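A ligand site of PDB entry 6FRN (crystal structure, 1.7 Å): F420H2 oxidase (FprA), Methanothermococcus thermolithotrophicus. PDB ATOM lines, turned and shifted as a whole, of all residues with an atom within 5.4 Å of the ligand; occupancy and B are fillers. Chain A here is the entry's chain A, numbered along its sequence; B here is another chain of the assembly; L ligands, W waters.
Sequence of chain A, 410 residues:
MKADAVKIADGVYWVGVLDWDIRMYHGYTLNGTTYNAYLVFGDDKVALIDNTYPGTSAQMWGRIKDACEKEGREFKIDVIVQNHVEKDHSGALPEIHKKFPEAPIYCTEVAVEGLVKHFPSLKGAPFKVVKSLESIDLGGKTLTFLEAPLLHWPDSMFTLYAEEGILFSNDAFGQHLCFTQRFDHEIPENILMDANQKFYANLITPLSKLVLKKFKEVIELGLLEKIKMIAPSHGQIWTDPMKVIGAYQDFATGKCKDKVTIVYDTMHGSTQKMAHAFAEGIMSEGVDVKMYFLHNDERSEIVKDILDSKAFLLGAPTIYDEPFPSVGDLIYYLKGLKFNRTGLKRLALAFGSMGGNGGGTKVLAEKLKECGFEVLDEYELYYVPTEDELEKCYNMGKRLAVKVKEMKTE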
ATOM      1  N   ASP A 265      28.764 -16.887 -10.873  1.00  0.00           N
ATOM      2  CA  ASP A 265      29.647 -17.322  -9.795  1.00  0.00           C
ATOM      3  C   ASP A 265      28.844 -18.237  -8.871  1.00  0.00           C
ATOM      4  O   ASP A 265      27.618 -18.241  -8.943  1.00  0.00           O
ATOM      5  CB  ASP A 265      30.351 -16.205  -9.014  1.00  0.00           C
ATOM      6  CG  ASP A 265      31.766 -16.587  -8.520  1.00  0.00           C
ATOM      7  OD1 ASP A 265      32.041 -17.802  -8.372  1.00  0.00           O
ATOM      8  OD2 ASP A 265      32.594 -15.674  -8.322  1.00  0.00           O
ATOM      9  N   THR A 266      29.526 -19.042  -8.053  1.00  0.00           N
ATOM     10  CA  THR A 266      28.864 -20.008  -7.167  1.00  0.00           C
ATOM     11  C   THR A 266      29.772 -20.290  -5.982  1.00  0.00           C
ATOM     12  O   THR A 266      30.987 -20.191  -6.096  1.00  0.00           O
ATOM     13  CB  THR A 266      28.542 -21.305  -7.946  1.00  0.00           C
ATOM     14  OG1 THR A 266      27.595 -22.094  -7.220  1.00  0.00           O
ATOM     15  CG2 THR A 266      29.770 -22.172  -8.212  1.00  0.00           C
ATOM     16  N   MET A 267      29.178 -20.587  -4.856  1.00  0.00           N
ATOM     17  CA  MET A 267      29.871 -20.999  -3.639  1.00  0.00           C
ATOM     18  C   MET A 267      29.788 -22.531  -3.446  1.00  0.00           C
ATOM     19  O   MET A 267      30.802 -23.163  -3.137  1.00  0.00           O
ATOM     20  CB  MET A 267      29.305 -20.282  -2.421  1.00  0.00           C
ATOM     21  CG  MET A 267      29.388 -18.778  -2.532  1.00  0.00           C
ATOM     22  SD  MET A 267      28.769 -17.912  -1.072  1.00  0.00           S
ATOM     23  CE  MET A 267      27.014 -18.203  -1.206  1.00  0.00           C
ATOM     24  N   HIS A 268      28.578 -23.088  -3.597  1.00  0.00           N
ATOM     25  CA  HIS A 268      28.292 -24.523  -3.429  1.00  0.00           C
ATOM     26  C   HIS A 268      27.900 -25.276  -4.709  1.00  0.00           C
ATOM     27  O   HIS A 268      27.647 -26.470  -4.643  1.00  0.00           O
ATOM     28  CB  HIS A 268      27.206 -24.718  -2.375  1.00  0.00           C
ATOM     29  CG  HIS A 268      27.508 -24.189  -1.006  1.00  0.00           C
ATOM     30  ND1 HIS A 268      28.610 -24.625  -0.288  1.00  0.00           N
ATOM     31  CD2 HIS A 268      26.775 -23.368  -0.215  1.00  0.00           C
ATOM     32  CE1 HIS A 268      28.506 -24.080   0.910  1.00  0.00           C
ATOM     33  NE2 HIS A 268      27.446 -23.272   0.992  1.00  0.00           N
ATOM     34  N   GLY A 269      27.804 -24.592  -5.843  1.00  0.00           N
ATOM     35  CA  GLY A 269      27.492 -25.204  -7.134  1.00  0.00           C
ATOM     36  C   GLY A 269      26.079 -25.100  -7.672  1.00  0.00           C
ATOM     37  O   GLY A 269      25.851 -25.432  -8.842  1.00  0.00           O
ATOM     38  N   SER A 270      25.123 -24.597  -6.896  1.00  0.00           N
ATOM     39  CA  SER A 270      23.719 -24.530  -7.372  1.00  0.00           C
ATOM     40  C   SER A 270      23.510 -23.534  -8.519  1.00  0.00           C
ATOM     41  O   SER A 270      22.847 -23.878  -9.509  1.00  0.00           O
ATOM     42  CB  SER A 270      22.784 -24.258  -6.220  1.00  0.00           C
ATOM     43  OG  SER A 270      22.820 -25.415  -5.390  1.00  0.00           O
ATOM     44  N   THR A 271      24.123 -22.346  -8.428  1.00  0.00           N
ATOM     45  CA  THR A 271      24.021 -21.364  -9.510  1.00  0.00           C
ATOM     46  C   THR A 271      24.662 -21.881 -10.753  1.00  0.00           C
ATOM     47  O   THR A 271      24.165 -21.605 -11.849  1.00  0.00           O
ATOM     48  CB  THR A 271      24.555 -20.008  -9.052  1.00  0.00           C
ATOM     49  OG1 THR A 271      23.798 -19.603  -7.906  1.00  0.00           O
ATOM     50  CG2 THR A 271      24.410 -18.954 -10.112  1.00  0.00           C
ATOM     51  N   GLN A 272      25.745 -22.676 -10.616  1.00  0.00           N
ATOM     52  CA  GLN A 272      26.387 -23.313 -11.770  1.00  0.00           C
ATOM     53  C   GLN A 272      25.417 -24.252 -12.471  1.00  0.00           C
ATOM     54  O   GLN A 272      25.298 -24.234 -13.701  1.00  0.00           O
ATOM     55  CB  GLN A 272      27.617 -24.097 -11.302  1.00  0.00           C
ATOM     56  CG  GLN A 272      28.310 -24.864 -12.385  1.00  0.00           C
ATOM     57  CD  GLN A 272      29.529 -25.524 -11.822  1.00  0.00           C
ATOM     58  OE1 GLN A 272      29.438 -26.616 -11.280  1.00  0.00           O
ATOM     59  NE2 GLN A 272      30.639 -24.796 -11.727  1.00  0.00           N
ATOM     60  N   PRO A 317      24.773 -16.485  -6.394  1.00  0.00           N
ATOM     61  CA  PRO A 317      24.015 -16.713  -5.166  1.00  0.00           C
ATOM     62  C   PRO A 317      23.974 -15.476  -4.276  1.00  0.00           C
ATOM     63  O   PRO A 317      24.765 -14.542  -4.449  1.00  0.00           O
ATOM     64  CB  PRO A 317      24.809 -17.816  -4.508  1.00  0.00           C
ATOM     65  CG  PRO A 317      26.207 -17.508  -4.857  1.00  0.00           C
ATOM     66  CD  PRO A 317      26.116 -17.089  -6.310  1.00  0.00           C
ATOM     67  N   THR A 318      23.102 -15.521  -3.235  1.00  0.00           N
ATOM     68  CA  THR A 318      23.013 -14.446  -2.287  1.00  0.00           C
ATOM     69  C   THR A 318      23.917 -14.708  -1.102  1.00  0.00           C
ATOM     70  O   THR A 318      23.955 -15.833  -0.579  1.00  0.00           O
ATOM     71  CB  THR A 318      21.569 -14.258  -1.800  1.00  0.00           C
ATOM     72  OG1 THR A 318      20.783 -13.926  -2.937  1.00  0.00           O
ATOM     73  CG2 THR A 318      21.427 -13.162  -0.774  1.00  0.00           C
ATOM     74  N   ILE A 319      24.642 -13.679  -0.683  1.00  0.00           N
ATOM     75  CA  ILE A 319      25.528 -13.700   0.468  1.00  0.00           C
ATOM     76  C   ILE A 319      25.266 -12.384   1.204  1.00  0.00           C
ATOM     77  O   ILE A 319      25.437 -11.316   0.612  1.00  0.00           O
ATOM     78  CB  ILE A 319      27.021 -13.957   0.060  1.00  0.00           C
ATOM     79  CG1 ILE A 319      28.008 -13.719   1.229  1.00  0.00           C
ATOM     80  CG2 ILE A 319      27.437 -13.149  -1.142  1.00  0.00           C
ATOM     81  CD1 ILE A 319      29.407 -14.373   0.963  1.00  0.00           C
ATOM     82  N   TYR A 320      24.722 -12.472   2.410  1.00  0.00           N
ATOM     83  CA  TYR A 320      24.348 -11.333   3.226  1.00  0.00           C
ATOM     84  C   TYR A 320      23.559 -10.274   2.418  1.00  0.00           C
ATOM     85  O   TYR A 320      23.941  -9.113   2.335  1.00  0.00           O
ATOM     86  CB  TYR A 320      25.555 -10.780   3.966  1.00  0.00           C
ATOM     87  CG  TYR A 320      25.849 -11.653   5.163  1.00  0.00           C
ATOM     88  CD1 TYR A 320      24.882 -11.886   6.130  1.00  0.00           C
ATOM     89  CD2 TYR A 320      27.057 -12.339   5.263  1.00  0.00           C
ATOM     90  CE1 TYR A 320      25.113 -12.704   7.212  1.00  0.00           C
ATOM     91  CE2 TYR A 320      27.308 -13.184   6.364  1.00  0.00           C
ATOM     92  CZ  TYR A 320      26.327 -13.358   7.329  1.00  0.00           C
ATOM     93  OH  TYR A 320      26.411 -14.137   8.452  1.00  0.00           O
ATOM     94  N   ASP A 321      22.450 -10.739   1.820  1.00  0.00           N
ATOM     95  CA  ASP A 321      21.473  -9.947   1.079  1.00  0.00           C
ATOM     96  C   ASP A 321      21.958  -9.393  -0.229  1.00  0.00           C
ATOM     97  O   ASP A 321      21.162  -8.753  -0.897  1.00  0.00           O
ATOM     98  CB  ASP A 321      20.936  -8.782   1.949  1.00  0.00           C
ATOM     99  CG  ASP A 321      20.504  -9.199   3.321  1.00  0.00           C
ATOM    100  OD1 ASP A 321      19.804 -10.217   3.435  1.00  0.00           O
ATOM    101  OD2 ASP A 321      20.918  -8.543   4.299  1.00  0.00           O
ATOM    102  N   SER A 353      20.822 -18.799  -6.704  1.00  0.00           N
ATOM    103  CA  SER A 353      20.319 -19.630  -5.619  1.00  0.00           C
ATOM    104  C   SER A 353      20.465 -18.861  -4.302  1.00  0.00           C
ATOM    105  O   SER A 353      21.317 -17.987  -4.197  1.00  0.00           O
ATOM    106  CB  SER A 353      21.078 -20.965  -5.590  1.00  0.00           C
ATOM    107  OG  SER A 353      20.642 -21.771  -4.506  1.00  0.00           O
ATOM    108  N   MET A 354      19.662 -19.209  -3.313  1.00  0.00           N
ATOM    109  CA  MET A 354      19.644 -18.539  -1.994  1.00  0.00           C
ATOM    110  C   MET A 354      19.327 -19.575  -0.935  1.00  0.00           C
ATOM    111  O   MET A 354      18.839 -20.649  -1.246  1.00  0.00           O
ATOM    112  CB  MET A 354      18.513 -17.462  -1.980  1.00  0.00           C
ATOM    113  CG  MET A 354      17.194 -18.012  -2.459  1.00  0.00           C
ATOM    114  SD  MET A 354      15.740 -17.070  -2.080  1.00  0.00           S
ATOM    115  CE  MET A 354      14.499 -18.036  -3.011  1.00  0.00           C
ATOM    116  N   GLY A 355      19.621 -19.246   0.306  1.00  0.00           N
ATOM    117  CA  GLY A 355      19.314 -20.113   1.455  1.00  0.00           C
ATOM    118  C   GLY A 355      18.305 -19.544   2.437  1.00  0.00           C
ATOM    119  O   GLY A 355      17.880 -20.251   3.350  1.00  0.00           O
ATOM    120  N   GLY A 356      17.938 -18.278   2.300  1.00  0.00           N
ATOM    121  CA  GLY A 356      17.023 -17.618   3.221  1.00  0.00           C
ATOM    122  C   GLY A 356      16.186 -16.555   2.563  1.00  0.00           C
ATOM    123  O   GLY A 356      15.301 -16.872   1.768  1.00  0.00           O
ATOM    124  N   ASN A 357      16.465 -15.282   2.873  1.00  0.00           N
ATOM    125  CA  ASN A 357      15.706 -14.169   2.311  1.00  0.00           C
ATOM    126  C   ASN A 357      16.020 -13.893   0.855  1.00  0.00           C
ATOM    127  O   ASN A 357      15.227 -13.273   0.177  1.00  0.00           O
ATOM    128  CB  ASN A 357      15.905 -12.899   3.130  1.00  0.00           C
ATOM    129  CG  ASN A 357      15.276 -12.991   4.502  1.00  0.00           C
ATOM    130  OD1 ASN A 357      14.098 -13.297   4.624  1.00  0.00           O
ATOM    131  ND2 ASN A 357      15.993 -12.664   5.545  1.00  0.00           N
ATOM    132  N   GLY A 358      17.170 -14.314   0.348  1.00  0.00           N
ATOM    133  CA  GLY A 358      17.502 -14.022  -1.041  1.00  0.00           C
ATOM    134  C   GLY A 358      17.715 -12.544  -1.271  1.00  0.00           C
ATOM    135  O   GLY A 358      18.088 -11.827  -0.341  1.00  0.00           O
ATOM    136  N   TYR A 382      15.722 -21.875  -4.140  1.00  0.00           N
ATOM    137  CA  TYR A 382      16.210 -22.258  -2.811  1.00  0.00           C
ATOM    138  C   TYR A 382      17.212 -23.407  -2.883  1.00  0.00           C
ATOM    139  O   TYR A 382      16.848 -24.498  -3.334  1.00  0.00           O
ATOM    140  CB  TYR A 382      15.003 -22.683  -1.978  1.00  0.00           C
ATOM    141  CG  TYR A 382      15.313 -23.146  -0.576  1.00  0.00           C
ATOM    142  CD1 TYR A 382      16.119 -22.394   0.264  1.00  0.00           C
ATOM    143  CD2 TYR A 382      14.700 -24.285  -0.052  1.00  0.00           C
ATOM    144  CE1 TYR A 382      16.292 -22.756   1.599  1.00  0.00           C
ATOM    145  CE2 TYR A 382      14.874 -24.659   1.274  1.00  0.00           C
ATOM    146  CZ  TYR A 382      15.664 -23.890   2.105  1.00  0.00           C
ATOM    147  OH  TYR A 382      15.854 -24.260   3.407  1.00  0.00           O
ATOM    148  N   TYR A 383      18.444 -23.185  -2.430  1.00  0.00           N
ATOM    149  CA  TYR A 383      19.502 -24.226  -2.395  1.00  0.00           C
ATOM    150  C   TYR A 383      19.634 -24.994  -3.725  1.00  0.00           C
ATOM    151  O   TYR A 383      19.758 -24.361  -4.789  1.00  0.00           O
ATOM    152  CB  TYR A 383      19.326 -25.174  -1.191  1.00  0.00           C
ATOM    153  CG  TYR A 383      19.519 -24.537   0.168  1.00  0.00           C
ATOM    154  CD1 TYR A 383      20.627 -23.723   0.419  1.00  0.00           C
ATOM    155  CD2 TYR A 383      18.702 -24.855   1.238  1.00  0.00           C
ATOM    156  CE1 TYR A 383      20.877 -23.218   1.697  1.00  0.00           C
ATOM    157  CE2 TYR A 383      18.947 -24.372   2.518  1.00  0.00           C
ATOM    158  CZ  TYR A 383      20.006 -23.509   2.733  1.00  0.00           C
ATOM    159  OH  TYR A 383      20.251 -22.996   3.990  1.00  0.00           O
ATOM    160  N   VAL A 384      19.638 -26.347  -3.699  1.00  0.00           N
ATOM    161  CA  VAL A 384      19.937 -27.144  -4.880  1.00  0.00           C
ATOM    162  C   VAL A 384      18.703 -27.215  -5.758  1.00  0.00           C
ATOM    163  O   VAL A 384      17.644 -27.647  -5.282  1.00  0.00           O
ATOM    164  CB  VAL A 384      20.418 -28.561  -4.457  1.00  0.00           C
ATOM    165  CG1 VAL A 384      20.781 -29.397  -5.677  1.00  0.00           C
ATOM    166  CG2 VAL A 384      21.610 -28.477  -3.502  1.00  0.00           C
ATOM    167  N   HIS B  26      33.942 -20.125  -0.537  1.00  0.00           N
ATOM    168  CA  HIS B  26      33.031 -18.995  -0.752  1.00  0.00           C
ATOM    169  C   HIS B  26      33.757 -17.650  -0.769  1.00  0.00           C
ATOM    170  O   HIS B  26      33.269 -16.678  -0.229  1.00  0.00           O
ATOM    171  CB  HIS B  26      31.829 -18.984   0.195  1.00  0.00           C
ATOM    172  CG  HIS B  26      32.166 -18.875   1.647  1.00  0.00           C
ATOM    173  ND1 HIS B  26      32.503 -17.663   2.225  1.00  0.00           N
ATOM    174  CD2 HIS B  26      32.166 -19.832   2.591  1.00  0.00           C
ATOM    175  CE1 HIS B  26      32.782 -17.942   3.498  1.00  0.00           C
ATOM    176  NE2 HIS B  26      32.595 -19.239   3.753  1.00  0.00           N
ATOM    177  N   GLU B  86      23.810 -26.264   5.920  1.00  0.00           N
ATOM    178  CA  GLU B  86      24.860 -26.084   4.944  1.00  0.00           C
ATOM    179  C   GLU B  86      25.717 -27.351   4.781  1.00  0.00           C
ATOM    180  O   GLU B  86      25.976 -28.054   5.749  1.00  0.00           O
ATOM    181  CB  GLU B  86      25.702 -24.848   5.219  1.00  0.00           C
ATOM    182  CG  GLU B  86      26.286 -24.828   6.608  1.00  0.00           C
ATOM    183  CD  GLU B  86      27.309 -23.730   6.732  1.00  0.00           C
ATOM    184  OE1 GLU B  86      27.325 -22.818   5.880  1.00  0.00           O
ATOM    185  OE2 GLU B  86      28.093 -23.800   7.710  1.00  0.00           O
ATOM    186  N   HIS B 152      19.029 -15.046  13.076  1.00  0.00           N
ATOM    187  CA  HIS B 152      19.031 -14.800  11.640  1.00  0.00           C
ATOM    188  C   HIS B 152      18.907 -16.013  10.785  1.00  0.00           C
ATOM    189  O   HIS B 152      18.375 -15.880   9.663  1.00  0.00           O
ATOM    190  CB  HIS B 152      20.270 -13.996  11.243  1.00  0.00           C
ATOM    191  CG  HIS B 152      20.141 -13.357   9.914  1.00  0.00           C
ATOM    192  ND1 HIS B 152      19.248 -12.315   9.691  1.00  0.00           N
ATOM    193  CD2 HIS B 152      20.784 -13.634   8.757  1.00  0.00           C
ATOM    194  CE1 HIS B 152      19.367 -12.007   8.416  1.00  0.00           C
ATOM    195  NE2 HIS B 152      20.284 -12.760   7.815  1.00  0.00           N
ATOM    196  N   TRP B 153      19.494 -17.170  11.195  1.00  0.00           N
ATOM    197  CA  TRP B 153      19.460 -18.382  10.386  1.00  0.00           C
ATOM    198  C   TRP B 153      18.499 -19.361  11.025  1.00  0.00           C
ATOM    199  O   TRP B 153      18.848 -19.981  12.025  1.00  0.00           O
ATOM    200  CB  TRP B 153      20.865 -19.000  10.207  1.00  0.00           C
ATOM    201  CG  TRP B 153      21.886 -18.076   9.664  1.00  0.00           C
ATOM    202  CD1 TRP B 153      23.063 -17.729  10.260  1.00  0.00           C
ATOM    203  CD2 TRP B 153      21.820 -17.317   8.439  1.00  0.00           C
ATOM    204  NE1 TRP B 153      23.787 -16.901   9.434  1.00  0.00           N
ATOM    205  CE2 TRP B 153      23.023 -16.594   8.337  1.00  0.00           C
ATOM    206  CE3 TRP B 153      20.885 -17.211   7.411  1.00  0.00           C
ATOM    207  CZ2 TRP B 153      23.308 -15.761   7.255  1.00  0.00           C
ATOM    208  CZ3 TRP B 153      21.161 -16.379   6.341  1.00  0.00           C
ATOM    209  CH2 TRP B 153      22.348 -15.638   6.291  1.00  0.00           C
ATOM    210  N   LEU B 203      31.963 -13.213   8.420  1.00  0.00           N
ATOM    211  CA  LEU B 203      30.715 -13.973   8.633  1.00  0.00           C
ATOM    212  C   LEU B 203      29.803 -13.482   9.717  1.00  0.00           C
ATOM    213  O   LEU B 203      28.634 -13.922   9.714  1.00  0.00           O
ATOM    214  CB  LEU B 203      31.096 -15.438   8.892  1.00  0.00           C
ATOM    215  CG  LEU B 203      31.904 -16.098   7.775  1.00  0.00           C
ATOM    216  CD1 LEU B 203      32.561 -17.340   8.240  1.00  0.00           C
ATOM    217  CD2 LEU B 203      31.052 -16.297   6.531  1.00  0.00           C
HETATM  218  N1  LIG L   1      21.354 -16.925   1.630  1.00  0.00           N
HETATM  219  C1  LIG L   1      20.453 -15.957   1.749  1.00  0.00           C
HETATM  220  O1  LIG L   1      19.342 -16.150   1.315  1.00  0.00           O
HETATM  221  N2  LIG L   1      20.733 -14.789   2.299  1.00  0.00           N
HETATM  222  C2  LIG L   1      21.926 -14.514   2.775  1.00  0.00           C
HETATM  223  O2  LIG L   1      22.136 -13.446   3.271  1.00  0.00           O
HETATM  224  C3  LIG L   1      22.998 -15.535   2.674  1.00  0.00           C
HETATM  225  N3  LIG L   1      24.230 -15.354   3.130  1.00  0.00           N
HETATM  226  C4  LIG L   1      25.156 -16.296   3.006  1.00  0.00           C
HETATM  227  C5  LIG L   1      26.443 -16.093   3.452  1.00  0.00           C
HETATM  228  C6  LIG L   1      27.401 -17.059   3.305  1.00  0.00           C
HETATM  229  C7  LIG L   1      28.799 -16.838   3.813  1.00  0.00           C
HETATM  230  C8  LIG L   1      27.065 -18.343   2.700  1.00  0.00           C
HETATM  231  C9  LIG L   1      28.092 -19.416   2.569  1.00  0.00           C
HETATM  232  C10 LIG L   1      25.769 -18.559   2.246  1.00  0.00           C
HETATM  233  C11 LIG L   1      24.805 -17.585   2.373  1.00  0.00           C
HETATM  234  N4  LIG L   1      23.527 -17.797   1.907  1.00  0.00           N
HETATM  235  C12 LIG L   1      22.600 -16.793   2.047  1.00  0.00           C
HETATM  236  C13 LIG L   1      23.114 -19.047   1.322  1.00  0.00           C
HETATM  237  C14 LIG L   1      23.372 -19.226  -0.147  1.00  0.00           C
HETATM  238  O3  LIG L   1      22.767 -18.183  -0.810  1.00  0.00           O
HETATM  239  C15 LIG L   1      22.834 -20.582  -0.564  1.00  0.00           C
HETATM  240  O4  LIG L   1      23.648 -21.560   0.012  1.00  0.00           O
HETATM  241  C16 LIG L   1      22.774 -20.845  -2.058  1.00  0.00           C
HETATM  242  O5  LIG L   1      22.095 -22.041  -2.240  1.00  0.00           O
HETATM  243  C17 LIG L   1      24.163 -20.945  -2.633  1.00  0.00           C
HETATM  244  O6  LIG L   1      24.237 -21.082  -4.025  1.00  0.00           O
HETATM  245  P1  LIG L   1      25.520 -21.651  -4.674  1.00  0.00           P
HETATM  246  O7  LIG L   1      25.433 -23.038  -4.439  1.00  0.00           O
HETATM  247  O8  LIG L   1      25.337 -21.271  -6.050  1.00  0.00           O
HETATM  248  O9  LIG L   1      26.638 -21.019  -4.048  1.00  0.00           O
HETATM  249  O   HOH W   1      23.585 -24.341  -3.023  1.00  0.00           O
HETATM  250  O   HOH W   2      20.462 -12.622   5.192  1.00  0.00           O
HETATM  251  O   HOH W   3      19.164 -12.423   2.095  1.00  0.00           O
HETATM  252  O   HOH W   4      26.246 -22.102   3.344  1.00  0.00           O
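An oxygen (O9) of the ligand lies within hydrogen-bond range of the backbone NH of Met 267, 2.7 Å away.
N of Thr 271 sits at hydrogen-bond distance from O8 of the ligand (2.9 Å).
OG of Ser 353 lies within hydrogen-bond range of O5 of the ligand (2.7 Å).
The side-chain hydroxyl of Thr 266 lies within hydrogen-bond range of an oxygen (O8) of the ligand, at 2.7 Å.
N of Asn 357 sits at hydrogen-bond distance from O1 of the ligand (3.4 Å).
An oxygen (O1) of the ligand sits at hydrogen-bond distance from the backbone NH (N) of Gly 356 (2.7 Å).
The backbone NH (N) of His 268 lies within hydrogen-bond range of an oxygen (O9) of the ligand, 2.9 Å away.
An oxygen (O7) of the ligand lies within hydrogen-bond range of the backbone NH (N) of Ser 270.
The backbone NH (N) of Gly 355 sits at hydrogen-bond distance from a nitrogen (N1) of the ligand (3.2 Å).
The backbone carbonyl oxygen (O) of Thr 318 is in hydrogen-bond range of an oxygen (O3) of the ligand, 2.6 Å away.
O8 of the ligand sits at hydrogen-bond distance from OG1 of Thr 271.
The backbone NH of Gly 358 lies within hydrogen-bond range of an oxygen (O1) of the ligand (3.0 Å).
N of Tyr 320 lies within hydrogen-bond range of O2 of the ligand, 2.9 Å away.
The backbone NH (N) of Gly 269 is in hydrogen-bond range of an oxygen (O7) of the ligand.
N of Asp 321 lies within hydrogen-bond range of O2 of the ligand.
O of Met 354 sits at hydrogen-bond distance from N of Tyr 383 (2.8 Å).
OG1 of Thr 266 sits at hydrogen-bond distance from N of Gly 269 (2.9 Å).
The side-chain hydroxyl (OG) of Ser 270 sits at hydrogen-bond distance from the backbone carbonyl oxygen (O) of Tyr 383 (3.3 Å).
The backbone NH (N) of Thr 318 is in hydrogen-bond range of the backbone carbonyl oxygen (O) of Ser 353 (3.2 Å).
OG of Ser 353 is in hydrogen-bond range of O of Tyr 383.
OG1 of Thr 271 lies within hydrogen-bond range of N of Ser 353, 3.3 Å away.
The side-chain hydroxyl (OH) of Tyr 320 lies within hydrogen-bond range of the backbone carbonyl oxygen (O) of Leu 203 of chain B.
CB of Pro 317 touches O6 of the ligand, at 3.4 Å.
Ile 319 touches the ligand (CA to N3, 3.4 Å).
Met 354 touches the ligand.
Tyr 383 touches the ligand.
CH2 of Trp 153 of chain B touches C3 of the ligand (3.7 Å).
Leu 203 of chain B touches the ligand (CD2 to C7, 3.6 Å).
Hydrophobic or aromatic side chains that line the ligand: Met 267, His 268, Pro 317, Ile 319, Met 354, Tyr 383, Trp 153 of chain B and Leu 203 of chain B.
Along chain A the residues within 4 Å of the ligand span positions 266 to 383.
The nearest printed residue that does not touch the ligand is His 26 of chain B (4.1 Å).
Water W1 lies within hydrogen-bond range of an oxygen (O7) of the ligand (2.7 Å) and the side-chain hydroxyl (OG) of Ser 270 (2.7 Å).
Water W2 lies within hydrogen-bond range of NE2 of His 152 of chain B (2.6 Å), O2 of the ligand (2.7 Å) and OD1 of Asp 321 (3.1 Å).
Water W3 lies within hydrogen-bond range of OD1 of Asp 321 (2.7 Å), O of Gly 358 (2.7 Å) and N2 of the ligand (2.8 Å).
Water W4 lies within hydrogen-bond range of OE1 of Glu 86 of chain B (2.8 Å) and NE2 of His 268 (2.9 Å).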
